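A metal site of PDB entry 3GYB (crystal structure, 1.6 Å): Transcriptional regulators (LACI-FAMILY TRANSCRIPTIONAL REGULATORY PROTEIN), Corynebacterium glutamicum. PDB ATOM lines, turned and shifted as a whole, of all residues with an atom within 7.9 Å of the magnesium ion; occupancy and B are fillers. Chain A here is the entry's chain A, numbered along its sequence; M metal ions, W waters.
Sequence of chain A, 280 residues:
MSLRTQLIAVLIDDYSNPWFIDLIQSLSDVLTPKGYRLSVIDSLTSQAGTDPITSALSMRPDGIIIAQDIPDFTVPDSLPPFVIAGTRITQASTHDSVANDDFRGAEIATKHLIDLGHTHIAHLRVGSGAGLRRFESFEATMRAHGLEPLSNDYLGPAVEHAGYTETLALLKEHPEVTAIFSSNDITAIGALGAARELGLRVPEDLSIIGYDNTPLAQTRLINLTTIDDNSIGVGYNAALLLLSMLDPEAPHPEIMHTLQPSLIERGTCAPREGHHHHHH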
ATOM      1  N   PRO A  18      23.334  15.666  15.400  1.00  0.00           N
ATOM      2  CA  PRO A  18      23.670  16.700  14.419  1.00  0.00           C
ATOM      3  C   PRO A  18      23.879  18.130  14.913  1.00  0.00           C
ATOM      4  O   PRO A  18      23.837  19.063  14.111  1.00  0.00           O
ATOM      5  CB  PRO A  18      22.524  16.609  13.415  1.00  0.00           C
ATOM      6  CG  PRO A  18      21.366  16.321  14.306  1.00  0.00           C
ATOM      7  CD  PRO A  18      21.924  15.253  15.243  1.00  0.00           C
ATOM      8  N   TRP A  19      24.112  18.309  16.211  1.00  0.00           N
ATOM      9  CA  TRP A  19      24.320  19.649  16.748  1.00  0.00           C
ATOM     10  C   TRP A  19      25.534  20.349  16.121  1.00  0.00           C
ATOM     11  O   TRP A  19      25.569  21.579  15.987  1.00  0.00           O
ATOM     12  CB  TRP A  19      24.526  19.592  18.262  1.00  0.00           C
ATOM     13  CG  TRP A  19      25.945  19.227  18.657  1.00  0.00           C
ATOM     14  CD1 TRP A  19      26.500  17.982  18.675  1.00  0.00           C
ATOM     15  CD2 TRP A  19      26.990  20.141  18.999  1.00  0.00           C
ATOM     16  NE1 TRP A  19      27.835  18.057  18.998  1.00  0.00           N
ATOM     17  CE2 TRP A  19      28.164  19.380  19.204  1.00  0.00           C
ATOM     18  CE3 TRP A  19      27.060  21.528  19.142  1.00  0.00           C
ATOM     19  CZ2 TRP A  19      29.383  19.954  19.549  1.00  0.00           C
ATOM     20  CZ3 TRP A  19      28.281  22.111  19.492  1.00  0.00           C
ATOM     21  CH2 TRP A  19      29.421  21.327  19.687  1.00  0.00           C
ATOM     22  N   PHE A  20      26.533  19.549  15.739  1.00  0.00           N
ATOM     23  CA  PHE A  20      27.793  20.050  15.193  1.00  0.00           C
ATOM     24  C   PHE A  20      27.837  20.370  13.705  1.00  0.00           C
ATOM     25  O   PHE A  20      28.777  21.020  13.239  1.00  0.00           O
ATOM     26  CB  PHE A  20      28.871  19.003  15.470  1.00  0.00           C
ATOM     27  CG  PHE A  20      28.683  17.735  14.684  1.00  0.00           C
ATOM     28  CD1 PHE A  20      29.208  17.618  13.398  1.00  0.00           C
ATOM     29  CD2 PHE A  20      27.918  16.697  15.182  1.00  0.00           C
ATOM     30  CE1 PHE A  20      28.960  16.481  12.621  1.00  0.00           C
ATOM     31  CE2 PHE A  20      27.662  15.556  14.415  1.00  0.00           C
ATOM     32  CZ  PHE A  20      28.188  15.447  13.134  1.00  0.00           C
ATOM     33  N   ILE A  21      26.833  19.938  12.957  1.00  0.00           N
ATOM     34  CA  ILE A  21      26.835  20.150  11.517  1.00  0.00           C
ATOM     35  C   ILE A  21      27.057  21.582  11.028  1.00  0.00           C
ATOM     36  O   ILE A  21      27.973  21.818  10.248  1.00  0.00           O
ATOM     37  CB  ILE A  21      25.577  19.549  10.864  1.00  0.00           C
ATOM     38  CG1 ILE A  21      25.572  18.022  11.096  1.00  0.00           C
ATOM     39  CG2 ILE A  21      25.556  19.840   9.367  1.00  0.00           C
ATOM     40  CD1 ILE A  21      24.395  17.289  10.454  1.00  0.00           C
ATOM     41  N   ASP A  22      26.240  22.531  11.459  1.00  0.00           N
ATOM     42  CA  ASP A  22      26.459  23.896  10.991  1.00  0.00           C
ATOM     43  C   ASP A  22      27.656  24.559  11.673  1.00  0.00           C
ATOM     44  O   ASP A  22      28.143  25.599  11.216  1.00  0.00           O
ATOM     45  CB  ASP A  22      25.189  24.762  11.094  1.00  0.00           C
ATOM     46  CG  ASP A  22      24.654  24.895  12.504  1.00  0.00           C
ATOM     47  OD1 ASP A  22      25.430  24.773  13.465  1.00  0.00           O
ATOM     48  OD2 ASP A  22      23.439  25.163  12.641  1.00  0.00           O
ATOM     49  N   LEU A  23      28.145  23.961  12.759  1.00  0.00           N
ATOM     50  CA  LEU A  23      29.322  24.501  13.444  1.00  0.00           C
ATOM     51  C   LEU A  23      30.529  24.174  12.556  1.00  0.00           C
ATOM     52  O   LEU A  23      31.400  25.012  12.338  1.00  0.00           O
ATOM     53  CB  LEU A  23      29.487  23.858  14.827  1.00  0.00           C
ATOM     54  CG  LEU A  23      30.641  24.364  15.713  1.00  0.00           C
ATOM     55  CD1 LEU A  23      30.329  24.058  17.169  1.00  0.00           C
ATOM     56  CD2 LEU A  23      31.953  23.725  15.295  1.00  0.00           C
ATOM     57  N   ASP A 185      18.189  18.876  21.319  1.00  0.00           N
ATOM     58  CA  ASP A 185      17.261  18.407  20.292  1.00  0.00           C
ATOM     59  C   ASP A 185      17.164  16.906  20.112  1.00  0.00           C
ATOM     60  O   ASP A 185      16.074  16.365  19.989  1.00  0.00           O
ATOM     61  CB  ASP A 185      17.605  19.031  18.937  1.00  0.00           C
ATOM     62  CG  ASP A 185      17.241  20.498  18.849  1.00  0.00           C
ATOM     63  OD1 ASP A 185      16.676  21.053  19.817  1.00  0.00           O
ATOM     64  OD2 ASP A 185      17.504  21.091  17.772  1.00  0.00           O
ATOM     65  N   TYR A 211      17.024  22.213  22.381  1.00  0.00           N
ATOM     66  CA  TYR A 211      18.186  23.096  22.442  1.00  0.00           C
ATOM     67  C   TYR A 211      19.195  22.620  21.401  1.00  0.00           C
ATOM     68  O   TYR A 211      19.510  21.429  21.348  1.00  0.00           O
ATOM     69  CB  TYR A 211      18.809  23.004  23.848  1.00  0.00           C
ATOM     70  CG  TYR A 211      19.649  24.199  24.285  1.00  0.00           C
ATOM     71  CD1 TYR A 211      19.329  24.907  25.449  1.00  0.00           C
ATOM     72  CD2 TYR A 211      20.771  24.600  23.562  1.00  0.00           C
ATOM     73  CE1 TYR A 211      20.105  25.969  25.877  1.00  0.00           C
ATOM     74  CE2 TYR A 211      21.569  25.668  23.992  1.00  0.00           C
ATOM     75  CZ  TYR A 211      21.225  26.347  25.153  1.00  0.00           C
ATOM     76  OH  TYR A 211      22.003  27.404  25.590  1.00  0.00           O
ATOM     77  N   ASP A 212      19.644  23.550  20.557  1.00  0.00           N
ATOM     78  CA  ASP A 212      20.629  23.333  19.488  1.00  0.00           C
ATOM     79  C   ASP A 212      20.184  23.794  18.105  1.00  0.00           C
ATOM     80  O   ASP A 212      21.014  24.142  17.292  1.00  0.00           O
ATOM     81  CB  ASP A 212      21.048  21.857  19.337  1.00  0.00           C
ATOM     82  CG  ASP A 212      21.928  21.366  20.464  1.00  0.00           C
ATOM     83  OD1 ASP A 212      22.406  22.191  21.264  1.00  0.00           O
ATOM     84  OD2 ASP A 212      22.129  20.134  20.549  1.00  0.00           O
ATOM     85  N   ASN A 213      18.886  23.808  17.838  1.00  0.00           N
ATOM     86  CA  ASN A 213      18.390  24.170  16.509  1.00  0.00           C
ATOM     87  C   ASN A 213      19.121  23.337  15.452  1.00  0.00           C
ATOM     88  O   ASN A 213      19.689  23.869  14.481  1.00  0.00           O
ATOM     89  CB  ASN A 213      18.570  25.647  16.186  1.00  0.00           C
ATOM     90  CG  ASN A 213      17.855  26.019  14.885  1.00  0.00           C
ATOM     91  OD1 ASN A 213      16.744  25.567  14.642  1.00  0.00           O
ATOM     92  ND2 ASN A 213      18.500  26.842  14.054  1.00  0.00           N
ATOM     93  N   THR A 214      19.102  22.027  15.666  1.00  0.00           N
ATOM     94  CA  THR A 214      19.713  21.067  14.758  1.00  0.00           C
ATOM     95  C   THR A 214      18.926  21.091  13.446  1.00  0.00           C
ATOM     96  O   THR A 214      17.816  21.609  13.400  1.00  0.00           O
ATOM     97  CB  THR A 214      19.580  19.639  15.297  1.00  0.00           C
ATOM     98  OG1 THR A 214      18.200  19.375  15.584  1.00  0.00           O
ATOM     99  CG2 THR A 214      20.413  19.433  16.550  1.00  0.00           C
ATOM    100  N   PRO A 215      19.507  20.541  12.376  1.00  0.00           N
ATOM    101  CA  PRO A 215      18.802  20.525  11.092  1.00  0.00           C
ATOM    102  C   PRO A 215      17.480  19.751  11.244  1.00  0.00           C
ATOM    103  O   PRO A 215      16.486  20.070  10.607  1.00  0.00           O
ATOM    104  CB  PRO A 215      19.788  19.806  10.173  1.00  0.00           C
ATOM    105  CG  PRO A 215      21.116  20.236  10.714  1.00  0.00           C
ATOM    106  CD  PRO A 215      20.907  20.109  12.211  1.00  0.00           C
ATOM    107  N   GLN A 218      14.663  21.785  12.330  1.00  0.00           N
ATOM    108  CA  GLN A 218      14.259  22.668  11.241  1.00  0.00           C
ATOM    109  C   GLN A 218      13.327  22.042  10.208  1.00  0.00           C
ATOM    110  O   GLN A 218      12.718  22.748   9.410  1.00  0.00           O
ATOM    111  CB  GLN A 218      15.513  23.182  10.519  1.00  0.00           C
ATOM    112  CG  GLN A 218      16.450  23.999  11.404  1.00  0.00           C
ATOM    113  CD  GLN A 218      17.789  24.230  10.737  1.00  0.00           C
ATOM    114  OE1 GLN A 218      17.861  24.488   9.532  1.00  0.00           O
ATOM    115  NE2 GLN A 218      18.866  24.152  11.519  1.00  0.00           N
ATOM    116  N   THR A 226      12.977  25.331  19.702  1.00  0.00           N
ATOM    117  CA  THR A 226      14.274  25.057  20.309  1.00  0.00           C
ATOM    118  C   THR A 226      15.066  26.318  20.593  1.00  0.00           C
ATOM    119  O   THR A 226      14.748  27.399  20.095  1.00  0.00           O
ATOM    120  CB  THR A 226      15.072  24.149  19.329  1.00  0.00           C
ATOM    121  OG1 THR A 226      16.353  23.811  19.868  1.00  0.00           O
ATOM    122  CG2 THR A 226      15.267  24.889  17.996  1.00  0.00           C
ATOM    123  N   ILE A 227      16.111  26.175  21.400  1.00  0.00           N
ATOM    124  CA  ILE A 227      16.987  27.288  21.720  1.00  0.00           C
ATOM    125  C   ILE A 227      18.154  27.241  20.748  1.00  0.00           C
ATOM    126  O   ILE A 227      18.867  26.240  20.665  1.00  0.00           O
ATOM    127  CB  ILE A 227      17.541  27.185  23.150  1.00  0.00           C
ATOM    128  CG1 ILE A 227      16.402  27.246  24.173  1.00  0.00           C
ATOM    129  CG2 ILE A 227      18.585  28.280  23.386  1.00  0.00           C
ATOM    130  CD1 ILE A 227      15.531  28.494  24.076  1.00  0.00           C
ATOM    131  N   ASP A 228      18.345  28.319  19.989  1.00  0.00           N
ATOM    132  CA  ASP A 228      19.458  28.397  19.056  1.00  0.00           C
ATOM    133  C   ASP A 228      20.719  28.543  19.918  1.00  0.00           C
ATOM    134  O   ASP A 228      20.827  29.486  20.695  1.00  0.00           O
ATOM    135  CB  ASP A 228      19.295  29.630  18.156  1.00  0.00           C
ATOM    136  CG  ASP A 228      20.281  29.670  17.010  1.00  0.00           C
ATOM    137  OD1 ASP A 228      21.350  29.047  17.118  1.00  0.00           O
ATOM    138  OD2 ASP A 228      19.973  30.345  16.003  1.00  0.00           O
ATOM    139  N   ASP A 229      21.653  27.595  19.794  1.00  0.00           N
ATOM    140  CA  ASP A 229      22.891  27.633  20.566  1.00  0.00           C
ATOM    141  C   ASP A 229      23.963  28.429  19.823  1.00  0.00           C
ATOM    142  O   ASP A 229      25.143  28.391  20.193  1.00  0.00           O
ATOM    143  CB  ASP A 229      23.400  26.211  20.846  1.00  0.00           C
ATOM    144  CG  ASP A 229      23.792  25.468  19.576  1.00  0.00           C
ATOM    145  OD1 ASP A 229      23.257  25.840  18.520  1.00  0.00           O
ATOM    146  OD2 ASP A 229      24.614  24.530  19.641  1.00  0.00           O
ATOM    147  N   ASN A 230      23.551  29.140  18.779  1.00  0.00           N
ATOM    148  CA  ASN A 230      24.453  29.948  17.980  1.00  0.00           C
ATOM    149  C   ASN A 230      25.666  29.117  17.548  1.00  0.00           C
ATOM    150  O   ASN A 230      26.800  29.607  17.582  1.00  0.00           O
ATOM    151  CB  ASN A 230      24.923  31.164  18.777  1.00  0.00           C
ATOM    152  CG  ASN A 230      25.219  32.365  17.902  1.00  0.00           C
ATOM    153  OD1 ASN A 230      25.661  32.220  16.759  1.00  0.00           O
ATOM    154  ND2 ASN A 230      24.966  33.557  18.430  1.00  0.00           N
ATOM    155  N   SER A 231      25.435  27.876  17.136  1.00  0.00           N
ATOM    156  CA  SER A 231      26.537  27.018  16.723  1.00  0.00           C
ATOM    157  C   SER A 231      27.260  27.569  15.495  1.00  0.00           C
ATOM    158  O   SER A 231      28.414  27.250  15.257  1.00  0.00           O
ATOM    159  CB  SER A 231      26.018  25.597  16.461  1.00  0.00           C
ATOM    160  OG  SER A 231      24.820  25.623  15.709  1.00  0.00           O
ATOM    161  N   ILE A 232      26.581  28.397  14.703  1.00  0.00           N
ATOM    162  CA  ILE A 232      27.217  28.994  13.543  1.00  0.00           C
ATOM    163  C   ILE A 232      28.214  30.035  14.028  1.00  0.00           C
ATOM    164  O   ILE A 232      29.356  30.105  13.557  1.00  0.00           O
ATOM    165  CB  ILE A 232      26.185  29.642  12.598  1.00  0.00           C
ATOM    166  CG1 ILE A 232      25.322  28.548  11.955  1.00  0.00           C
ATOM    167  CG2 ILE A 232      26.895  30.465  11.530  1.00  0.00           C
ATOM    168  CD1 ILE A 232      24.127  29.072  11.211  1.00  0.00           C
ATOM    169  N   GLY A 233      27.792  30.837  15.002  1.00  0.00           N
ATOM    170  CA  GLY A 233      28.666  31.860  15.559  1.00  0.00           C
ATOM    171  C   GLY A 233      29.839  31.236  16.285  1.00  0.00           C
ATOM    172  O   GLY A 233      30.957  31.756  16.268  1.00  0.00           O
ATOM    173  N   ILE A 264      13.791  30.011  19.195  1.00  0.00           N
ATOM    174  CA  ILE A 264      13.259  29.860  17.853  1.00  0.00           C
ATOM    175  C   ILE A 264      11.946  29.129  18.050  1.00  0.00           C
ATOM    176  O   ILE A 264      11.931  27.954  18.418  1.00  0.00           O
ATOM    177  CB  ILE A 264      14.173  29.012  16.940  1.00  0.00           C
ATOM    178  CG1 ILE A 264      15.511  29.714  16.724  1.00  0.00           C
ATOM    179  CG2 ILE A 264      13.482  28.798  15.592  1.00  0.00           C
ATOM    180  CD1 ILE A 264      16.466  28.952  15.831  1.00  0.00           C
HETATM  181 MG    MG M   1      22.933  24.913  16.653  1.00  0.00          MG
HETATM  182  O   HOH W   1      22.393  24.054  14.663  1.00  0.00           O
HETATM  183  O   HOH W   2      23.995  23.134  17.436  1.00  0.00           O
HETATM  184  O   HOH W   3      21.991  26.763  16.022  1.00  0.00           O
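The nearest printed residue that does not touch the magnesium ion is Asn 213 (4.04 Å).
Water W1 lies within hydrogen-bond range of the side-chain carboxylate of Asp 22 (2.5 Å) and the backbone carbonyl oxygen of Asn 213 (2.7 Å). Water W2 bridges the backbone carbonyl oxygen (O) of Trp 19 (2.6 Å) and the side-chain carboxylate (OD2) of Asp 229 (2.7 Å).
The magnesium ion is bound by OD1 of Asp 229, 2.1 Å away. The magnesium ion is bound by O of Asp 212, at 2.2 Å. The magnesium ion is bound by water W3, 2.2 Å away. Water W2 binds the magnesium ion. OG of Ser 231 is bound to the magnesium ion. The magnesium ion is bound by water W1 (2.2 Å). The magnesium ion has six donor atoms within binding distance.
The backbone NH (N) of Asp 212 is in hydrogen-bond range of the backbone carbonyl oxygen (O) of Ile 227, 2.8 Å away. The side-chain hydroxyl (OG1) of Thr 226 lies within hydrogen-bond range of the backbone NH (N) of Asp 212, 3.4 Å away. OD1 of Asp 22 lies close to OG of Ser 231 (2.5 Å).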
